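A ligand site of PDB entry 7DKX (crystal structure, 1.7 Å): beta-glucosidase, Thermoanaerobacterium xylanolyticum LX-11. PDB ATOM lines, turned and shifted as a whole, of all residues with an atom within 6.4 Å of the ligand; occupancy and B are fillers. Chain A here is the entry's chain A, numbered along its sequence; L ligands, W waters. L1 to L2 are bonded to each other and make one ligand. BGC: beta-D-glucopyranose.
The side-chain carboxylate (OD1) of Asp 578 sits at hydrogen-bond distance from the side-chain amide nitrogen (NE2) of Gln 712 (3.1 Å).
OD2 of Asp 578 sits at hydrogen-bond distance from OH of Tyr 508 (2.6 Å).
The indole nitrogen of Trp 510 is in hydrogen-bond range of the backbone carbonyl oxygen of Asp 578 (3.1 Å).
The side-chain hydroxyl (OH) of Tyr 430 is in hydrogen-bond range of the guanidinium group (NH1) of Arg 771.
O of Arg 771 is in hydrogen-bond range of N of Glu 762 (3.3 Å).
N of Thr 579 is in hydrogen-bond range of OE1 of Gln 712 (3.0 Å).
The side-chain hydroxyl (OH) of Tyr 430 lies within hydrogen-bond range of the side-chain hydroxyl (OH) of Tyr 47, at 2.7 Å.
OH of Tyr 47 touches O4 of BGC L1 (3.6 Å).
Tyr 430 touches the ligand.
Tyr 508 touches the ligand.
Trp 510 touches the ligand.
CG2 of Thr 579 touches O2 of BGC L2 (3.5 Å).
NE2 of Gln 712 touches O3 of BGC L2 (3.5 Å).
Hydrophobic or aromatic side chains that line the ligand: Tyr 47, Tyr 430, Tyr 508 and Trp 510.
Of the 17 residues printed, 8 come within 4 Å of the ligand.
Along chain A the residues within 4 Å of the ligand span positions 47 to 771.
Water W7 lies within hydrogen-bond range of O2 of BGC L2 (2.8 Å), OG1 of Thr 579 (2.9 Å) and NE2 of Gln 712 (3.1 Å).
Water W3 lies within hydrogen-bond range of O6 of BGC L2 (2.8 Å), OH of Tyr 432 (2.8 Å), N of Asp 509 (3.1 Å) and N of Trp 510 (3.2 Å).
Water W2 bridges the side-chain hydroxyl (OH) of Tyr 47 (2.6 Å) and an oxygen (O2) of BGC L2 (2.8 Å).
Water W6 lies within hydrogen-bond range of OE2 of Glu 762 (2.7 Å), NH2 of Arg 771 (2.9 Å) and O3 of BGC L2 (3.4 Å).
An oxygen (O4) of BGC L2 is in hydrogen-bond range of the side-chain carboxylate (OD2) of Asp 578 (2.6 Å).
The guanidinium group (NH1) of Arg 771 is in hydrogen-bond range of an oxygen (O3) of BGC L2 (3.1 Å).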
ATOM      1  N   TYR A  47     -27.389  27.682  26.492  1.00  0.00           N
ATOM      2  CA  TYR A  47     -28.166  28.095  25.340  1.00  0.00           C
ATOM      3  C   TYR A  47     -29.620  27.676  25.596  1.00  0.00           C
ATOM      4  O   TYR A  47     -29.864  26.854  26.494  1.00  0.00           O
ATOM      5  CB  TYR A  47     -27.596  27.527  24.038  1.00  0.00           C
ATOM      6  CG  TYR A  47     -27.407  26.028  24.002  1.00  0.00           C
ATOM      7  CD1 TYR A  47     -26.232  25.443  24.500  1.00  0.00           C
ATOM      8  CD2 TYR A  47     -28.387  25.195  23.480  1.00  0.00           C
ATOM      9  CE1 TYR A  47     -26.043  24.054  24.473  1.00  0.00           C
ATOM     10  CE2 TYR A  47     -28.205  23.818  23.450  1.00  0.00           C
ATOM     11  CZ  TYR A  47     -27.036  23.250  23.961  1.00  0.00           C
ATOM     12  OH  TYR A  47     -26.845  21.878  23.935  1.00  0.00           O
ATOM     13  N   ASP A 429     -34.793  19.569  20.211  1.00  0.00           N
ATOM     14  CA  ASP A 429     -33.749  20.602  20.357  1.00  0.00           C
ATOM     15  C   ASP A 429     -32.721  20.523  19.239  1.00  0.00           C
ATOM     16  O   ASP A 429     -32.223  21.556  18.794  1.00  0.00           O
ATOM     17  CB  ASP A 429     -33.015  20.485  21.676  1.00  0.00           C
ATOM     18  CG  ASP A 429     -33.875  20.857  22.877  1.00  0.00           C
ATOM     19  OD1 ASP A 429     -34.217  22.040  23.042  1.00  0.00           O
ATOM     20  OD2 ASP A 429     -34.175  19.956  23.686  1.00  0.00           O
ATOM     21  N   TYR A 430     -32.406  19.307  18.831  1.00  0.00           N
ATOM     22  CA  TYR A 430     -31.497  19.020  17.724  1.00  0.00           C
ATOM     23  C   TYR A 430     -32.356  18.328  16.656  1.00  0.00           C
ATOM     24  O   TYR A 430     -32.455  17.087  16.583  1.00  0.00           O
ATOM     25  CB  TYR A 430     -30.318  18.157  18.219  1.00  0.00           C
ATOM     26  CG  TYR A 430     -29.685  18.573  19.546  1.00  0.00           C
ATOM     27  CD1 TYR A 430     -29.462  19.914  19.892  1.00  0.00           C
ATOM     28  CD2 TYR A 430     -29.265  17.609  20.458  1.00  0.00           C
ATOM     29  CE1 TYR A 430     -28.843  20.256  21.096  1.00  0.00           C
ATOM     30  CE2 TYR A 430     -28.661  17.941  21.653  1.00  0.00           C
ATOM     31  CZ  TYR A 430     -28.439  19.266  21.974  1.00  0.00           C
ATOM     32  OH  TYR A 430     -27.824  19.533  23.183  1.00  0.00           O
ATOM     33  N   TYR A 432     -33.259  16.856  13.833  1.00  0.00           N
ATOM     34  CA  TYR A 432     -32.750  16.081  12.697  1.00  0.00           C
ATOM     35  C   TYR A 432     -33.444  14.730  12.670  1.00  0.00           C
ATOM     36  O   TYR A 432     -33.575  14.101  13.723  1.00  0.00           O
ATOM     37  CB  TYR A 432     -31.221  15.908  12.831  1.00  0.00           C
ATOM     38  CG  TYR A 432     -30.552  17.247  13.128  1.00  0.00           C
ATOM     39  CD1 TYR A 432     -30.760  18.304  12.272  1.00  0.00           C
ATOM     40  CD2 TYR A 432     -29.772  17.466  14.267  1.00  0.00           C
ATOM     41  CE1 TYR A 432     -30.204  19.556  12.496  1.00  0.00           C
ATOM     42  CE2 TYR A 432     -29.214  18.733  14.516  1.00  0.00           C
ATOM     43  CZ  TYR A 432     -29.446  19.765  13.614  1.00  0.00           C
ATOM     44  OH  TYR A 432     -28.923  21.055  13.804  1.00  0.00           O
ATOM     45  N   HIS A 492     -25.225  11.782   8.591  1.00  0.00           N
ATOM     46  CA  HIS A 492     -25.631  11.895   9.987  1.00  0.00           C
ATOM     47  C   HIS A 492     -27.144  11.790  10.182  1.00  0.00           C
ATOM     48  O   HIS A 492     -27.596  11.236  11.193  1.00  0.00           O
ATOM     49  CB  HIS A 492     -25.136  13.227  10.526  1.00  0.00           C
ATOM     50  CG  HIS A 492     -25.559  13.515  11.931  1.00  0.00           C
ATOM     51  ND1 HIS A 492     -26.709  14.217  12.211  1.00  0.00           N
ATOM     52  CD2 HIS A 492     -24.970  13.263  13.126  1.00  0.00           C
ATOM     53  CE1 HIS A 492     -26.822  14.374  13.512  1.00  0.00           C
ATOM     54  NE2 HIS A 492     -25.780  13.799  14.089  1.00  0.00           N
ATOM     55  N   TYR A 508     -27.601  18.504  10.277  1.00  0.00           N
ATOM     56  CA  TYR A 508     -26.673  18.703  11.393  1.00  0.00           C
ATOM     57  C   TYR A 508     -25.385  19.364  10.901  1.00  0.00           C
ATOM     58  O   TYR A 508     -24.836  18.963   9.882  1.00  0.00           O
ATOM     59  CB  TYR A 508     -26.353  17.342  12.041  1.00  0.00           C
ATOM     60  CG  TYR A 508     -25.258  17.285  13.077  1.00  0.00           C
ATOM     61  CD1 TYR A 508     -25.511  17.466  14.429  1.00  0.00           C
ATOM     62  CD2 TYR A 508     -23.944  16.961  12.691  1.00  0.00           C
ATOM     63  CE1 TYR A 508     -24.499  17.350  15.377  1.00  0.00           C
ATOM     64  CE2 TYR A 508     -22.947  16.840  13.622  1.00  0.00           C
ATOM     65  CZ  TYR A 508     -23.213  17.041  14.951  1.00  0.00           C
ATOM     66  OH  TYR A 508     -22.181  16.915  15.829  1.00  0.00           O
ATOM     67  N   ASP A 509     -24.942  20.389  11.642  1.00  0.00           N
ATOM     68  CA  ASP A 509     -23.719  21.105  11.293  1.00  0.00           C
ATOM     69  C   ASP A 509     -22.769  21.422  12.439  1.00  0.00           C
ATOM     70  O   ASP A 509     -21.753  22.077  12.199  1.00  0.00           O
ATOM     71  CB  ASP A 509     -24.061  22.377  10.485  1.00  0.00           C
ATOM     72  CG  ASP A 509     -24.888  23.375  11.276  1.00  0.00           C
ATOM     73  OD1 ASP A 509     -25.057  23.233  12.493  1.00  0.00           O
ATOM     74  OD2 ASP A 509     -25.374  24.346  10.635  1.00  0.00           O
ATOM     75  N   TRP A 510     -23.022  20.943  13.669  1.00  0.00           N
ATOM     76  CA  TRP A 510     -22.134  21.185  14.803  1.00  0.00           C
ATOM     77  C   TRP A 510     -20.720  20.626  14.568  1.00  0.00           C
ATOM     78  O   TRP A 510     -19.718  21.269  14.929  1.00  0.00           O
ATOM     79  CB  TRP A 510     -22.724  20.642  16.111  1.00  0.00           C
ATOM     80  CG  TRP A 510     -21.824  20.720  17.258  1.00  0.00           C
ATOM     81  CD1 TRP A 510     -21.243  19.678  17.911  1.00  0.00           C
ATOM     82  CD2 TRP A 510     -21.324  21.903  17.872  1.00  0.00           C
ATOM     83  NE1 TRP A 510     -20.428  20.128  18.902  1.00  0.00           N
ATOM     84  CE2 TRP A 510     -20.456  21.496  18.905  1.00  0.00           C
ATOM     85  CE3 TRP A 510     -21.518  23.270  17.652  1.00  0.00           C
ATOM     86  CZ2 TRP A 510     -19.786  22.404  19.716  1.00  0.00           C
ATOM     87  CZ3 TRP A 510     -20.861  24.179  18.463  1.00  0.00           C
ATOM     88  CH2 TRP A 510     -20.010  23.744  19.487  1.00  0.00           C
ATOM     89  N   THR A 576     -20.467  10.140  17.712  1.00  0.00           N
ATOM     90  CA  THR A 576     -21.686  10.533  18.460  1.00  0.00           C
ATOM     91  C   THR A 576     -21.447  11.365  19.717  1.00  0.00           C
ATOM     92  O   THR A 576     -22.267  12.229  20.047  1.00  0.00           O
ATOM     93  CB  THR A 576     -22.533   9.272  18.803  1.00  0.00           C
ATOM     94  OG1 THR A 576     -23.901   9.653  19.053  1.00  0.00           O
ATOM     95  CG2 THR A 576     -21.962   8.507  19.964  1.00  0.00           C
ATOM     96  N   ASP A 578     -20.168  14.092  20.449  1.00  0.00           N
ATOM     97  CA  ASP A 578     -19.740  15.131  19.511  1.00  0.00           C
ATOM     98  C   ASP A 578     -19.198  16.408  20.174  1.00  0.00           C
ATOM     99  O   ASP A 578     -19.002  17.420  19.487  1.00  0.00           O
ATOM    100  CB  ASP A 578     -20.842  15.425  18.483  1.00  0.00           C
ATOM    101  CG  ASP A 578     -22.083  16.058  19.100  1.00  0.00           C
ATOM    102  OD1 ASP A 578     -22.262  15.985  20.345  1.00  0.00           O
ATOM    103  OD2 ASP A 578     -22.876  16.587  18.306  1.00  0.00           O
ATOM    104  N   THR A 579     -18.935  16.350  21.472  1.00  0.00           N
ATOM    105  CA  THR A 579     -18.024  17.304  22.111  1.00  0.00           C
ATOM    106  C   THR A 579     -16.852  16.615  22.832  1.00  0.00           C
ATOM    107  O   THR A 579     -16.008  17.305  23.365  1.00  0.00           O
ATOM    108  CB  THR A 579     -18.747  18.322  23.049  1.00  0.00           C
ATOM    109  OG1 THR A 579     -19.433  17.653  24.114  1.00  0.00           O
ATOM    110  CG2 THR A 579     -19.734  19.146  22.287  1.00  0.00           C
ATOM    111  N   ILE A 711     -17.690  17.898  29.119  1.00  0.00           N
ATOM    112  CA  ILE A 711     -19.032  17.729  29.702  1.00  0.00           C
ATOM    113  C   ILE A 711     -19.633  16.332  29.426  1.00  0.00           C
ATOM    114  O   ILE A 711     -20.239  15.730  30.318  1.00  0.00           O
ATOM    115  CB  ILE A 711     -19.995  18.861  29.233  1.00  0.00           C
ATOM    116  CG1 ILE A 711     -21.367  18.758  29.905  1.00  0.00           C
ATOM    117  CG2 ILE A 711     -20.164  18.878  27.703  1.00  0.00           C
ATOM    118  CD1 ILE A 711     -21.338  18.763  31.422  1.00  0.00           C
ATOM    119  N   GLN A 712     -19.470  15.820  28.205  1.00  0.00           N
ATOM    120  CA  GLN A 712     -20.066  14.514  27.860  1.00  0.00           C
ATOM    121  C   GLN A 712     -19.496  13.361  28.667  1.00  0.00           C
ATOM    122  O   GLN A 712     -20.211  12.405  28.998  1.00  0.00           O
ATOM    123  CB  GLN A 712     -19.969  14.251  26.362  1.00  0.00           C
ATOM    124  CG  GLN A 712     -20.894  15.165  25.571  1.00  0.00           C
ATOM    125  CD  GLN A 712     -20.797  14.995  24.082  1.00  0.00           C
ATOM    126  OE1 GLN A 712     -19.841  14.422  23.565  1.00  0.00           O
ATOM    127  NE2 GLN A 712     -21.773  15.533  23.363  1.00  0.00           N
ATOM    128  N   TRP A 717     -25.636   8.986  29.765  1.00  0.00           N
ATOM    129  CA  TRP A 717     -26.490   8.964  28.588  1.00  0.00           C
ATOM    130  C   TRP A 717     -27.486   7.837  28.775  1.00  0.00           C
ATOM    131  O   TRP A 717     -27.110   6.671  28.905  1.00  0.00           O
ATOM    132  CB  TRP A 717     -25.681   8.814  27.304  1.00  0.00           C
ATOM    133  CG  TRP A 717     -25.032  10.110  26.868  1.00  0.00           C
ATOM    134  CD1 TRP A 717     -24.824  11.223  27.632  1.00  0.00           C
ATOM    135  CD2 TRP A 717     -24.466  10.386  25.592  1.00  0.00           C
ATOM    136  NE1 TRP A 717     -24.186  12.181  26.892  1.00  0.00           N
ATOM    137  CE2 TRP A 717     -23.958  11.701  25.636  1.00  0.00           C
ATOM    138  CE3 TRP A 717     -24.379   9.663  24.406  1.00  0.00           C
ATOM    139  CZ2 TRP A 717     -23.347  12.302  24.527  1.00  0.00           C
ATOM    140  CZ3 TRP A 717     -23.776  10.253  23.301  1.00  0.00           C
ATOM    141  CH2 TRP A 717     -23.282  11.574  23.361  1.00  0.00           C
ATOM    142  N   GLU A 762     -31.579  12.882  26.611  1.00  0.00           N
ATOM    143  CA  GLU A 762     -30.290  12.279  26.273  1.00  0.00           C
ATOM    144  C   GLU A 762     -29.497  11.974  27.549  1.00  0.00           C
ATOM    145  O   GLU A 762     -29.012  10.857  27.733  1.00  0.00           O
ATOM    146  CB  GLU A 762     -29.455  13.236  25.400  1.00  0.00           C
ATOM    147  CG  GLU A 762     -27.980  12.845  25.209  1.00  0.00           C
ATOM    148  CD  GLU A 762     -27.746  11.861  24.078  1.00  0.00           C
ATOM    149  OE1 GLU A 762     -28.046  10.651  24.225  1.00  0.00           O
ATOM    150  OE2 GLU A 762     -27.203  12.285  23.018  1.00  0.00           O
ATOM    151  N   ARG A 771     -29.898  17.336  29.636  1.00  0.00           N
ATOM    152  CA  ARG A 771     -29.690  17.897  28.317  1.00  0.00           C
ATOM    153  C   ARG A 771     -30.553  17.126  27.327  1.00  0.00           C
ATOM    154  O   ARG A 771     -30.503  15.891  27.289  1.00  0.00           O
ATOM    155  CB  ARG A 771     -28.225  17.847  27.923  1.00  0.00           C
ATOM    156  CG  ARG A 771     -27.916  18.553  26.606  1.00  0.00           C
ATOM    157  CD  ARG A 771     -26.414  18.706  26.397  1.00  0.00           C
ATOM    158  NE  ARG A 771     -25.709  17.419  26.329  1.00  0.00           N
ATOM    159  CZ  ARG A 771     -25.543  16.687  25.227  1.00  0.00           C
ATOM    160  NH1 ARG A 771     -26.076  17.044  24.066  1.00  0.00           N
ATOM    161  NH2 ARG A 771     -24.870  15.552  25.290  1.00  0.00           N
ATOM    162  N   TYR A 775     -35.992  12.415  23.778  1.00  0.00           N
ATOM    163  CA  TYR A 775     -34.819  11.953  23.051  1.00  0.00           C
ATOM    164  C   TYR A 775     -34.993  10.525  22.536  1.00  0.00           C
ATOM    165  O   TYR A 775     -35.546   9.697  23.229  1.00  0.00           O
ATOM    166  CB  TYR A 775     -33.588  12.063  23.955  1.00  0.00           C
ATOM    167  CG  TYR A 775     -32.336  12.305  23.185  1.00  0.00           C
ATOM    168  CD1 TYR A 775     -32.030  13.573  22.702  1.00  0.00           C
ATOM    169  CD2 TYR A 775     -31.456  11.268  22.887  1.00  0.00           C
ATOM    170  CE1 TYR A 775     -30.899  13.805  21.945  1.00  0.00           C
ATOM    171  CE2 TYR A 775     -30.312  11.482  22.129  1.00  0.00           C
ATOM    172  CZ  TYR A 775     -30.027  12.749  21.682  1.00  0.00           C
ATOM    173  OH  TYR A 775     -28.903  12.987  20.930  1.00  0.00           O
HETATM  174  C2  BGC L   1     -24.052  25.592  20.081  1.00  0.00           C
HETATM  175  C3  BGC L   1     -24.652  24.208  20.374  1.00  0.00           C
HETATM  176  C4  BGC L   1     -23.600  23.316  21.033  1.00  0.00           C
HETATM  177  C5  BGC L   1     -22.902  24.031  22.190  1.00  0.00           C
HETATM  178  C6  BGC L   1     -21.672  23.302  22.716  1.00  0.00           C
HETATM  179  C1  BGC L   1     -23.494  26.183  21.376  1.00  0.00           C
HETATM  180  O1  BGC L   1     -22.906  27.475  21.189  1.00  0.00           O
HETATM  181  O2  BGC L   1     -25.064  26.419  19.524  1.00  0.00           O
HETATM  182  O3  BGC L   1     -25.144  23.627  19.165  1.00  0.00           O
HETATM  183  O4  BGC L   1     -24.219  22.142  21.553  1.00  0.00           O
HETATM  184  O5  BGC L   1     -22.436  25.336  21.804  1.00  0.00           O
HETATM  185  O6  BGC L   1     -21.386  23.728  24.051  1.00  0.00           O
HETATM  186  C2  BGC L   2     -24.238  19.789  21.616  1.00  0.00           C
HETATM  187  C3  BGC L   2     -24.172  18.535  20.751  1.00  0.00           C
HETATM  188  C4  BGC L   2     -25.324  18.588  19.748  1.00  0.00           C
HETATM  189  C5  BGC L   2     -25.240  19.892  18.930  1.00  0.00           C
HETATM  190  C6  BGC L   2     -26.371  20.042  17.915  1.00  0.00           C
HETATM  191  C1  BGC L   2     -24.154  20.997  20.723  1.00  0.00           C
HETATM  192  O2  BGC L   2     -23.153  19.819  22.542  1.00  0.00           O
HETATM  193  O3  BGC L   2     -24.189  17.392  21.634  1.00  0.00           O
HETATM  194  O4  BGC L   2     -25.286  17.471  18.862  1.00  0.00           O
HETATM  195  O5  BGC L   2     -25.249  21.013  19.808  1.00  0.00           O
HETATM  196  O6  BGC L   2     -26.199  21.256  17.169  1.00  0.00           O
HETATM  197  O   HOH W   1     -19.498  25.786  22.641  1.00  0.00           O
HETATM  198  O   HOH W   2     -24.415  21.151  24.633  1.00  0.00           O
HETATM  199  O   HOH W   3     -26.157  20.966  14.415  1.00  0.00           O
HETATM  200  O   HOH W   4     -22.428  25.818  25.295  1.00  0.00           O
HETATM  201  O   HOH W   5     -27.379  26.756  20.711  1.00  0.00           O
HETATM  202  O   HOH W   6     -25.434  14.355  22.694  1.00  0.00           O
HETATM  203  O   HOH W   7     -22.179  18.282  24.625  1.00  0.00           O
